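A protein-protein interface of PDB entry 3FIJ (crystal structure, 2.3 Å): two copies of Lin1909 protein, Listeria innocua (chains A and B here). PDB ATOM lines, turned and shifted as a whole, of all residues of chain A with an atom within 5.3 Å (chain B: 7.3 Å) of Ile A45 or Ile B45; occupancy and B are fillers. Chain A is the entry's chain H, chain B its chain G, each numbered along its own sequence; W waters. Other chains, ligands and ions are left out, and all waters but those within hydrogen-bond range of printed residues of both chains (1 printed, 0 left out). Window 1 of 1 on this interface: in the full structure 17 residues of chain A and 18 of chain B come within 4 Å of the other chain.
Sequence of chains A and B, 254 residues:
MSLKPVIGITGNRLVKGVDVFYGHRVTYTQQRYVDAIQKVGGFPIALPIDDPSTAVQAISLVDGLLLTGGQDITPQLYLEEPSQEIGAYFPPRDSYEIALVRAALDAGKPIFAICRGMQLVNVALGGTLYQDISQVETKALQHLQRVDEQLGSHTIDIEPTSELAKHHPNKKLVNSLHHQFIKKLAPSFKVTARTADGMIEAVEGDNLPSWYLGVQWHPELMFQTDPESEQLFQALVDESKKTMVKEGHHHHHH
Phe A43 touches Leu B61, and with the chains exchanged Leu A61 touches Phe B43. Ile A45 touches Leu B47, and with the chains exchanged Leu A47 touches Ile B45. Ala B46 touches its own counterpart, Ala A46. Leu A61 touches Ile B45, but with the chains exchanged Ile A45 does not touch Leu B61 (4.1 Å). Positions printed for both chains: 6, 7, 8, 9, 43, 44, 45, 46, 47, 48, 61 and 62. Of the 21 pairs that touch across the chains among the printed residues, 12 have their exchanged pair printed and touching as well.
The backbone NH (N) of Ile B7 lies within hydrogen-bond range of the backbone carbonyl oxygen (O) of Phe B43 (3.0 Å). The backbone NH (N) of Ile A7 lies within hydrogen-bond range of the backbone carbonyl oxygen (O) of Phe A43, 3.0 Å away. The backbone NH of Ile B9 lies within hydrogen-bond range of the backbone carbonyl oxygen of Ile B45 (2.7 Å). The backbone carbonyl oxygen (O) of Pro B5 is in hydrogen-bond range of the backbone NH (N) of Phe B43 (2.8 Å). The backbone NH of Ile A9 is in hydrogen-bond range of the backbone carbonyl oxygen of Ile A45, 2.7 Å away. The backbone carbonyl oxygen of Ile A7 sits at hydrogen-bond distance from the backbone NH of Ile A45 (2.9 Å).
The backbone NH (N) of Ala B46 lies within hydrogen-bond range of the backbone carbonyl oxygen (O) of Ala A46 (2.8 Å).
Of the printed residues of chain B, Ile A45 touches Ile B45 (3.3 Å), Ala B46 (3.8 Å), Leu B47 (3.4 Å) and Pro B48 (3.99 Å). Ile B45 touches just these residues of chain A: Ile A45, Ala A46, Leu A47 and Leu A61. Printed residues of chain A within 4 Å of Asp B50: Phe A43 and Pro A44. Of the printed residues of chain A, Leu B47 touches Ile A45 (3.4 Å). Printed residues of chain A within 4 Å of Gln B57: Val A6 and Phe A43. Of the printed residues of chain A, Ala B46 touches Ile A45 (3.8 Å) and Ala A46 (2.8 Å). Ile A7 touches none of the printed residues of chain B. The nearest residue of chain A that does not touch Ile B45 is Pro A48 (4.2 Å).
Water W1 lies within hydrogen-bond range of the backbone carbonyl oxygen (O) of Pro A44 and the side-chain carboxylate (OD2) of Asp B50.
Printed residues of chain A that touch a printed residue of chain B: Val A6, Phe A43, Pro A44, Ile A45, Ala A46, Leu A47, Pro A48 and Leu A61. Along chain A the printed residues that touch a printed residue of chain B span positions 6 to 61. Printed residues of chain B that touch a printed residue of chain A: Val B6, Val B34, Phe B43, Pro B44, Ile B45, Ala B46, Leu B47, Pro B48, Asp B50, Gln B57, Ala B58, Leu B61 and Tyr B96. Among the printed residues, no Asp or Glu carboxylate lies within 4 Å of a Lys or Arg side-chain nitrogen of the other chain.
Val A6 touches Gln B57. Phe A43 touches Gln B57. CE2 of Phe A43 touches CD1 of Leu B61 (3.8 Å). CZ of Phe A43 touches OH of Tyr B96 (3.7 Å). Pro B48 touches Pro A44 (CG to O, 3.4 Å). Ala A46 touches Ile B45 (O to C, 3.9 Å). Ile B45 touches Leu A47 (CD1 to CD2, 3.5 Å). Pro A48 touches Val B34 (CB to CG1, 3.8 Å). CD of Pro A48 touches O of Pro B44 (3.6 Å). Leu A61 touches Val B6 (CD1 to CG1, 3.9 Å).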
ATOM      1  N   VAL A   6      10.941   1.508  24.539  1.00  0.00           N
ATOM      2  CA  VAL A   6      11.824   0.439  24.981  1.00  0.00           C
ATOM      3  C   VAL A   6      11.295  -0.921  24.529  1.00  0.00           C
ATOM      4  O   VAL A   6      10.248  -1.379  24.998  1.00  0.00           O
ATOM      5  CB  VAL A   6      11.966   0.427  26.518  1.00  0.00           C
ATOM      6  CG1 VAL A   6      12.661  -0.860  26.972  1.00  0.00           C
ATOM      7  CG2 VAL A   6      12.749   1.652  26.976  1.00  0.00           C
ATOM      8  N   ILE A   7      12.016  -1.568  23.620  1.00  0.00           N
ATOM      9  CA  ILE A   7      11.596  -2.876  23.134  1.00  0.00           C
ATOM     10  C   ILE A   7      12.433  -4.003  23.734  1.00  0.00           C
ATOM     11  O   ILE A   7      13.647  -4.057  23.538  1.00  0.00           O
ATOM     12  CB  ILE A   7      11.690  -2.977  21.604  1.00  0.00           C
ATOM     13  CG1 ILE A   7      10.941  -1.814  20.949  1.00  0.00           C
ATOM     14  CG2 ILE A   7      11.093  -4.303  21.150  1.00  0.00           C
ATOM     15  CD1 ILE A   7       9.438  -1.839  21.183  1.00  0.00           C
ATOM     16  N   GLY A   8      11.779  -4.893  24.476  1.00  0.00           N
ATOM     17  CA  GLY A   8      12.482  -6.016  25.069  1.00  0.00           C
ATOM     18  C   GLY A   8      12.622  -7.120  24.036  1.00  0.00           C
ATOM     19  O   GLY A   8      11.627  -7.556  23.458  1.00  0.00           O
ATOM     20  N   ILE A   9      13.856  -7.556  23.791  1.00  0.00           N
ATOM     21  CA  ILE A   9      14.129  -8.613  22.824  1.00  0.00           C
ATOM     22  C   ILE A   9      14.560  -9.882  23.534  1.00  0.00           C
ATOM     23  O   ILE A   9      15.569  -9.914  24.244  1.00  0.00           O
ATOM     24  CB  ILE A   9      15.228  -8.203  21.829  1.00  0.00           C
ATOM     25  CG1 ILE A   9      14.798  -6.946  21.071  1.00  0.00           C
ATOM     26  CG2 ILE A   9      15.496  -9.339  20.857  1.00  0.00           C
ATOM     27  CD1 ILE A   9      15.820  -6.457  20.076  1.00  0.00           C
ATOM     28  N   PHE A  43      14.354   1.717  21.404  1.00  0.00           N
ATOM     29  CA  PHE A  43      15.560   1.465  22.180  1.00  0.00           C
ATOM     30  C   PHE A  43      15.478   0.012  22.618  1.00  0.00           C
ATOM     31  O   PHE A  43      14.710  -0.329  23.523  1.00  0.00           O
ATOM     32  CB  PHE A  43      15.632   2.346  23.418  1.00  0.00           C
ATOM     33  CG  PHE A  43      16.841   2.080  24.258  1.00  0.00           C
ATOM     34  CD1 PHE A  43      18.095   2.512  23.844  1.00  0.00           C
ATOM     35  CD2 PHE A  43      16.736   1.340  25.428  1.00  0.00           C
ATOM     36  CE1 PHE A  43      19.227   2.209  24.577  1.00  0.00           C
ATOM     37  CE2 PHE A  43      17.863   1.034  26.169  1.00  0.00           C
ATOM     38  CZ  PHE A  43      19.112   1.468  25.742  1.00  0.00           C
ATOM     39  N   PRO A  44      16.263  -0.866  21.976  1.00  0.00           N
ATOM     40  CA  PRO A  44      16.237  -2.284  22.329  1.00  0.00           C
ATOM     41  C   PRO A  44      16.990  -2.667  23.587  1.00  0.00           C
ATOM     42  O   PRO A  44      17.969  -2.041  23.980  1.00  0.00           O
ATOM     43  CB  PRO A  44      16.817  -2.954  21.088  1.00  0.00           C
ATOM     44  CG  PRO A  44      17.845  -1.952  20.640  1.00  0.00           C
ATOM     45  CD  PRO A  44      17.074  -0.644  20.764  1.00  0.00           C
ATOM     46  N   ILE A  45      16.499  -3.723  24.206  1.00  0.00           N
ATOM     47  CA  ILE A  45      17.084  -4.278  25.404  1.00  0.00           C
ATOM     48  C   ILE A  45      17.018  -5.786  25.188  1.00  0.00           C
ATOM     49  O   ILE A  45      16.094  -6.282  24.545  1.00  0.00           O
ATOM     50  CB  ILE A  45      16.250  -3.887  26.650  1.00  0.00           C
ATOM     51  CG1 ILE A  45      16.426  -2.397  26.946  1.00  0.00           C
ATOM     52  CG2 ILE A  45      16.671  -4.717  27.854  1.00  0.00           C
ATOM     53  CD1 ILE A  45      17.805  -2.026  27.415  1.00  0.00           C
ATOM     54  N   ALA A  46      18.001  -6.513  25.695  1.00  0.00           N
ATOM     55  CA  ALA A  46      17.995  -7.961  25.554  1.00  0.00           C
ATOM     56  C   ALA A  46      17.697  -8.575  26.916  1.00  0.00           C
ATOM     57  O   ALA A  46      18.426  -8.340  27.884  1.00  0.00           O
ATOM     58  CB  ALA A  46      19.346  -8.450  25.037  1.00  0.00           C
ATOM     59  N   LEU A  47      16.621  -9.353  26.992  1.00  0.00           N
ATOM     60  CA  LEU A  47      16.236  -9.996  28.245  1.00  0.00           C
ATOM     61  C   LEU A  47      16.814 -11.403  28.348  1.00  0.00           C
ATOM     62  O   LEU A  47      16.394 -12.316  27.640  1.00  0.00           O
ATOM     63  CB  LEU A  47      14.710 -10.061  28.359  1.00  0.00           C
ATOM     64  CG  LEU A  47      13.955  -8.739  28.181  1.00  0.00           C
ATOM     65  CD1 LEU A  47      12.457  -8.999  28.147  1.00  0.00           C
ATOM     66  CD2 LEU A  47      14.305  -7.782  29.312  1.00  0.00           C
ATOM     67  N   PRO A  48      17.786 -11.598  29.241  1.00  0.00           N
ATOM     68  CA  PRO A  48      18.406 -12.917  29.421  1.00  0.00           C
ATOM     69  C   PRO A  48      17.377 -13.928  29.927  1.00  0.00           C
ATOM     70  O   PRO A  48      16.272 -13.556  30.314  1.00  0.00           O
ATOM     71  CB  PRO A  48      19.484 -12.658  30.474  1.00  0.00           C
ATOM     72  CG  PRO A  48      19.743 -11.167  30.372  1.00  0.00           C
ATOM     73  CD  PRO A  48      18.377 -10.604  30.151  1.00  0.00           C
ATOM     74  N   LEU A  61       9.934  -3.215  32.582  1.00  0.00           N
ATOM     75  CA  LEU A  61      11.022  -2.397  32.070  1.00  0.00           C
ATOM     76  C   LEU A  61      10.797  -1.983  30.628  1.00  0.00           C
ATOM     77  O   LEU A  61      11.482  -1.093  30.128  1.00  0.00           O
ATOM     78  CB  LEU A  61      12.346  -3.152  32.157  1.00  0.00           C
ATOM     79  CG  LEU A  61      12.815  -3.532  33.558  1.00  0.00           C
ATOM     80  CD1 LEU A  61      14.166  -4.229  33.471  1.00  0.00           C
ATOM     81  CD2 LEU A  61      12.910  -2.272  34.426  1.00  0.00           C
ATOM     82  N   VAL A  62       9.825  -2.600  29.961  1.00  0.00           N
ATOM     83  CA  VAL A  62       9.597  -2.299  28.548  1.00  0.00           C
ATOM     84  C   VAL A  62       8.196  -1.885  28.110  1.00  0.00           C
ATOM     85  O   VAL A  62       7.208  -2.102  28.814  1.00  0.00           O
ATOM     86  CB  VAL A  62       9.998  -3.510  27.675  1.00  0.00           C
ATOM     87  CG1 VAL A  62      11.385  -4.002  28.070  1.00  0.00           C
ATOM     88  CG2 VAL A  62       8.955  -4.624  27.819  1.00  0.00           C
ATOM     89  N   PRO B   5      17.240  -5.384  42.150  1.00  0.00           N
ATOM     90  CA  PRO B   5      17.996  -4.330  41.460  1.00  0.00           C
ATOM     91  C   PRO B   5      18.245  -4.664  39.988  1.00  0.00           C
ATOM     92  O   PRO B   5      18.693  -5.759  39.665  1.00  0.00           O
ATOM     93  CB  PRO B   5      19.299  -4.260  42.256  1.00  0.00           C
ATOM     94  CG  PRO B   5      18.915  -4.773  43.606  1.00  0.00           C
ATOM     95  CD  PRO B   5      18.022  -5.931  43.270  1.00  0.00           C
ATOM     96  N   VAL B   6      17.945  -3.721  39.103  1.00  0.00           N
ATOM     97  CA  VAL B   6      18.160  -3.934  37.679  1.00  0.00           C
ATOM     98  C   VAL B   6      19.614  -3.624  37.341  1.00  0.00           C
ATOM     99  O   VAL B   6      20.043  -2.466  37.395  1.00  0.00           O
ATOM    100  CB  VAL B   6      17.257  -3.021  36.819  1.00  0.00           C
ATOM    101  CG1 VAL B   6      17.507  -3.287  35.342  1.00  0.00           C
ATOM    102  CG2 VAL B   6      15.794  -3.261  37.155  1.00  0.00           C
ATOM    103  N   ILE B   7      20.372  -4.665  37.007  1.00  0.00           N
ATOM    104  CA  ILE B   7      21.769  -4.495  36.643  1.00  0.00           C
ATOM    105  C   ILE B   7      21.916  -4.527  35.125  1.00  0.00           C
ATOM    106  O   ILE B   7      21.511  -5.492  34.473  1.00  0.00           O
ATOM    107  CB  ILE B   7      22.642  -5.607  37.248  1.00  0.00           C
ATOM    108  CG1 ILE B   7      22.556  -5.560  38.774  1.00  0.00           C
ATOM    109  CG2 ILE B   7      24.088  -5.441  36.782  1.00  0.00           C
ATOM    110  CD1 ILE B   7      22.979  -4.219  39.382  1.00  0.00           C
ATOM    111  N   GLY B   8      22.479  -3.461  34.565  1.00  0.00           N
ATOM    112  CA  GLY B   8      22.684  -3.403  33.129  1.00  0.00           C
ATOM    113  C   GLY B   8      24.003  -4.071  32.788  1.00  0.00           C
ATOM    114  O   GLY B   8      25.041  -3.731  33.365  1.00  0.00           O
ATOM    115  N   ILE B   9      23.958  -5.038  31.872  1.00  0.00           N
ATOM    116  CA  ILE B   9      25.154  -5.762  31.435  1.00  0.00           C
ATOM    117  C   ILE B   9      25.467  -5.377  29.992  1.00  0.00           C
ATOM    118  O   ILE B   9      24.647  -5.562  29.094  1.00  0.00           O
ATOM    119  CB  ILE B   9      24.951  -7.295  31.527  1.00  0.00           C
ATOM    120  CG1 ILE B   9      24.720  -7.694  32.986  1.00  0.00           C
ATOM    121  CG2 ILE B   9      26.164  -8.018  30.979  1.00  0.00           C
ATOM    122  CD1 ILE B   9      24.578  -9.174  33.211  1.00  0.00           C
ATOM    123  N   THR B  10      26.655  -4.829  29.774  1.00  0.00           N
ATOM    124  CA  THR B  10      27.059  -4.395  28.444  1.00  0.00           C
ATOM    125  C   THR B  10      27.447  -5.593  27.565  1.00  0.00           C
ATOM    126  O   THR B  10      28.059  -6.551  28.041  1.00  0.00           O
ATOM    127  CB  THR B  10      28.223  -3.381  28.548  1.00  0.00           C
ATOM    128  OG1 THR B  10      28.321  -2.637  27.328  1.00  0.00           O
ATOM    129  CG2 THR B  10      29.539  -4.098  28.841  1.00  0.00           C
ATOM    130  N   GLY B  11      27.088  -5.531  26.284  1.00  0.00           N
ATOM    131  CA  GLY B  11      27.374  -6.638  25.385  1.00  0.00           C
ATOM    132  C   GLY B  11      28.388  -6.431  24.276  1.00  0.00           C
ATOM    133  O   GLY B  11      29.012  -5.375  24.166  1.00  0.00           O
ATOM    134  N   VAL B  34      25.549 -12.961  33.537  1.00  0.00           N
ATOM    135  CA  VAL B  34      24.133 -13.074  33.866  1.00  0.00           C
ATOM    136  C   VAL B  34      24.004 -13.993  35.076  1.00  0.00           C
ATOM    137  O   VAL B  34      23.352 -13.643  36.061  1.00  0.00           O
ATOM    138  CB  VAL B  34      23.319 -13.665  32.685  1.00  0.00           C
ATOM    139  CG1 VAL B  34      21.904 -14.016  33.137  1.00  0.00           C
ATOM    140  CG2 VAL B  34      23.261 -12.659  31.548  1.00  0.00           C
ATOM    141  N   ILE B  37      24.930 -12.233  38.354  1.00  0.00           N
ATOM    142  CA  ILE B  37      23.922 -11.290  38.817  1.00  0.00           C
ATOM    143  C   ILE B  37      22.711 -12.002  39.415  1.00  0.00           C
ATOM    144  O   ILE B  37      22.335 -11.748  40.560  1.00  0.00           O
ATOM    145  CB  ILE B  37      23.437 -10.381  37.673  1.00  0.00           C
ATOM    146  CG1 ILE B  37      24.612  -9.576  37.116  1.00  0.00           C
ATOM    147  CG2 ILE B  37      22.334  -9.459  38.172  1.00  0.00           C
ATOM    148  CD1 ILE B  37      25.344  -8.754  38.159  1.00  0.00           C
ATOM    149  N   GLY B  42      20.297  -9.810  41.795  1.00  0.00           N
ATOM    150  CA  GLY B  42      19.942  -8.758  40.868  1.00  0.00           C
ATOM    151  C   GLY B  42      19.165  -9.308  39.693  1.00  0.00           C
ATOM    152  O   GLY B  42      19.096 -10.522  39.496  1.00  0.00           O
ATOM    153  N   PHE B  43      18.552  -8.414  38.931  1.00  0.00           N
ATOM    154  CA  PHE B  43      17.822  -8.801  37.732  1.00  0.00           C
ATOM    155  C   PHE B  43      18.652  -8.215  36.598  1.00  0.00           C
ATOM    156  O   PHE B  43      18.674  -6.997  36.389  1.00  0.00           O
ATOM    157  CB  PHE B  43      16.416  -8.203  37.693  1.00  0.00           C
ATOM    158  CG  PHE B  43      15.657  -8.547  36.444  1.00  0.00           C
ATOM    159  CD1 PHE B  43      15.243  -9.856  36.207  1.00  0.00           C
ATOM    160  CD2 PHE B  43      15.409  -7.578  35.471  1.00  0.00           C
ATOM    161  CE1 PHE B  43      14.593 -10.197  35.020  1.00  0.00           C
ATOM    162  CE2 PHE B  43      14.760  -7.908  34.277  1.00  0.00           C
ATOM    163  CZ  PHE B  43      14.356  -9.220  34.052  1.00  0.00           C
ATOM    164  N   PRO B  44      19.366  -9.078  35.862  1.00  0.00           N
ATOM    165  CA  PRO B  44      20.203  -8.623  34.749  1.00  0.00           C
ATOM    166  C   PRO B  44      19.416  -8.238  33.504  1.00  0.00           C
ATOM    167  O   PRO B  44      18.363  -8.793  33.221  1.00  0.00           O
ATOM    168  CB  PRO B  44      21.127  -9.812  34.518  1.00  0.00           C
ATOM    169  CG  PRO B  44      20.215 -10.976  34.798  1.00  0.00           C
ATOM    170  CD  PRO B  44      19.502 -10.534  36.064  1.00  0.00           C
ATOM    171  N   ILE B  45      19.956  -7.272  32.777  1.00  0.00           N
ATOM    172  CA  ILE B  45      19.377  -6.759  31.545  1.00  0.00           C
ATOM    173  C   ILE B  45      20.568  -6.606  30.603  1.00  0.00           C
ATOM    174  O   ILE B  45      21.610  -6.089  31.008  1.00  0.00           O
ATOM    175  CB  ILE B  45      18.724  -5.371  31.789  1.00  0.00           C
ATOM    176  CG1 ILE B  45      17.370  -5.544  32.486  1.00  0.00           C
ATOM    177  CG2 ILE B  45      18.577  -4.607  30.490  1.00  0.00           C
ATOM    178  CD1 ILE B  45      16.338  -6.292  31.671  1.00  0.00           C
ATOM    179  N   ALA B  46      20.435  -7.069  29.363  1.00  0.00           N
ATOM    180  CA  ALA B  46      21.533  -6.954  28.402  1.00  0.00           C
ATOM    181  C   ALA B  46      21.353  -5.676  27.605  1.00  0.00           C
ATOM    182  O   ALA B  46      20.307  -5.461  27.000  1.00  0.00           O
ATOM    183  CB  ALA B  46      21.554  -8.150  27.467  1.00  0.00           C
ATOM    184  N   LEU B  47      22.374  -4.826  27.617  1.00  0.00           N
ATOM    185  CA  LEU B  47      22.328  -3.564  26.892  1.00  0.00           C
ATOM    186  C   LEU B  47      23.085  -3.691  25.576  1.00  0.00           C
ATOM    187  O   LEU B  47      24.316  -3.636  25.543  1.00  0.00           O
ATOM    188  CB  LEU B  47      22.955  -2.447  27.732  1.00  0.00           C
ATOM    189  CG  LEU B  47      22.253  -2.118  29.051  1.00  0.00           C
ATOM    190  CD1 LEU B  47      23.103  -1.125  29.841  1.00  0.00           C
ATOM    191  CD2 LEU B  47      20.867  -1.550  28.773  1.00  0.00           C
ATOM    192  N   PRO B  48      22.357  -3.857  24.466  1.00  0.00           N
ATOM    193  CA  PRO B  48      23.048  -3.983  23.185  1.00  0.00           C
ATOM    194  C   PRO B  48      23.790  -2.699  22.835  1.00  0.00           C
ATOM    195  O   PRO B  48      23.551  -1.654  23.433  1.00  0.00           O
ATOM    196  CB  PRO B  48      21.912  -4.292  22.215  1.00  0.00           C
ATOM    197  CG  PRO B  48      20.753  -3.549  22.817  1.00  0.00           C
ATOM    198  CD  PRO B  48      20.895  -3.851  24.287  1.00  0.00           C
ATOM    199  N   ASP B  50      24.491   0.599  21.120  1.00  0.00           N
ATOM    200  CA  ASP B  50      23.586   1.595  20.545  1.00  0.00           C
ATOM    201  C   ASP B  50      24.351   2.914  20.376  1.00  0.00           C
ATOM    202  O   ASP B  50      25.549   2.978  20.645  1.00  0.00           O
ATOM    203  CB  ASP B  50      22.378   1.807  21.472  1.00  0.00           C
ATOM    204  CG  ASP B  50      21.119   2.247  20.718  1.00  0.00           C
ATOM    205  OD1 ASP B  50      21.212   3.157  19.861  1.00  0.00           O
ATOM    206  OD2 ASP B  50      20.030   1.683  20.988  1.00  0.00           O
ATOM    207  N   GLN B  57      19.249   7.195  28.354  1.00  0.00           N
ATOM    208  CA  GLN B  57      18.021   6.414  28.488  1.00  0.00           C
ATOM    209  C   GLN B  57      18.326   5.004  28.975  1.00  0.00           C
ATOM    210  O   GLN B  57      17.535   4.405  29.703  1.00  0.00           O
ATOM    211  CB  GLN B  57      17.265   6.338  27.158  1.00  0.00           C
ATOM    212  CG  GLN B  57      16.042   5.439  27.256  1.00  0.00           C
ATOM    213  CD  GLN B  57      15.112   5.533  26.069  1.00  0.00           C
ATOM    214  OE1 GLN B  57      14.078   4.870  26.039  1.00  0.00           O
ATOM    215  NE2 GLN B  57      15.467   6.356  25.087  1.00  0.00           N
ATOM    216  N   ALA B  58      19.473   4.473  28.570  1.00  0.00           N
ATOM    217  CA  ALA B  58      19.875   3.134  28.978  1.00  0.00           C
ATOM    218  C   ALA B  58      20.131   3.072  30.484  1.00  0.00           C
ATOM    219  O   ALA B  58      19.615   2.194  31.174  1.00  0.00           O
ATOM    220  CB  ALA B  58      21.130   2.707  28.213  1.00  0.00           C
ATOM    221  N   LEU B  61      17.327   3.133  33.007  1.00  0.00           N
ATOM    222  CA  LEU B  61      16.553   1.905  33.131  1.00  0.00           C
ATOM    223  C   LEU B  61      17.152   0.955  34.160  1.00  0.00           C
ATOM    224  O   LEU B  61      16.532  -0.046  34.517  1.00  0.00           O
ATOM    225  CB  LEU B  61      16.455   1.186  31.777  1.00  0.00           C
ATOM    226  CG  LEU B  61      15.820   1.929  30.594  1.00  0.00           C
ATOM    227  CD1 LEU B  61      15.842   1.038  29.356  1.00  0.00           C
ATOM    228  CD2 LEU B  61      14.393   2.324  30.926  1.00  0.00           C
ATOM    229  N   VAL B  62      18.342   1.281  34.656  1.00  0.00           N
ATOM    230  CA  VAL B  62      19.012   0.411  35.617  1.00  0.00           C
ATOM    231  C   VAL B  62      19.408   1.057  36.943  1.00  0.00           C
ATOM    232  O   VAL B  62      19.434   2.283  37.077  1.00  0.00           O
ATOM    233  CB  VAL B  62      20.282  -0.195  34.986  1.00  0.00           C
ATOM    234  CG1 VAL B  62      19.970  -0.689  33.571  1.00  0.00           C
ATOM    235  CG2 VAL B  62      21.403   0.843  34.965  1.00  0.00           C
ATOM    236  N   GLY B  64      22.204  -0.460  38.528  1.00  0.00           N
ATOM    237  CA  GLY B  64      23.626  -0.777  38.560  1.00  0.00           C
ATOM    238  C   GLY B  64      24.151  -1.078  37.164  1.00  0.00           C
ATOM    239  O   GLY B  64      23.390  -1.540  36.315  1.00  0.00           O
ATOM    240  N   LEU B  66      27.134  -3.087  34.868  1.00  0.00           N
ATOM    241  CA  LEU B  66      28.204  -4.082  34.814  1.00  0.00           C
ATOM    242  C   LEU B  66      28.896  -4.053  33.447  1.00  0.00           C
ATOM    243  O   LEU B  66      28.278  -4.338  32.417  1.00  0.00           O
ATOM    244  CB  LEU B  66      27.643  -5.479  35.086  1.00  0.00           C
ATOM    245  CG  LEU B  66      28.657  -6.629  35.148  1.00  0.00           C
ATOM    246  CD1 LEU B  66      29.728  -6.295  36.172  1.00  0.00           C
ATOM    247  CD2 LEU B  66      27.957  -7.944  35.504  1.00  0.00           C
ATOM    248  N   TYR B  96      29.855   3.834  22.804  1.00  0.00           N
ATOM    249  CA  TYR B  96      28.632   3.643  23.570  1.00  0.00           C
ATOM    250  C   TYR B  96      28.913   3.357  25.050  1.00  0.00           C
ATOM    251  O   TYR B  96      28.230   3.888  25.923  1.00  0.00           O
ATOM    252  CB  TYR B  96      27.797   2.511  22.960  1.00  0.00           C
ATOM    253  CG  TYR B  96      26.454   2.321  23.620  1.00  0.00           C
ATOM    254  CD1 TYR B  96      25.443   3.271  23.481  1.00  0.00           C
ATOM    255  CD2 TYR B  96      26.196   1.191  24.396  1.00  0.00           C
ATOM    256  CE1 TYR B  96      24.199   3.099  24.103  1.00  0.00           C
ATOM    257  CE2 TYR B  96      24.965   1.010  25.020  1.00  0.00           C
ATOM    258  CZ  TYR B  96      23.974   1.962  24.869  1.00  0.00           C
ATOM    259  OH  TYR B  96      22.763   1.767  25.478  1.00  0.00           O
HETATM  260  O   HOH W   1      20.035  -0.480  22.936  1.00  0.00           O
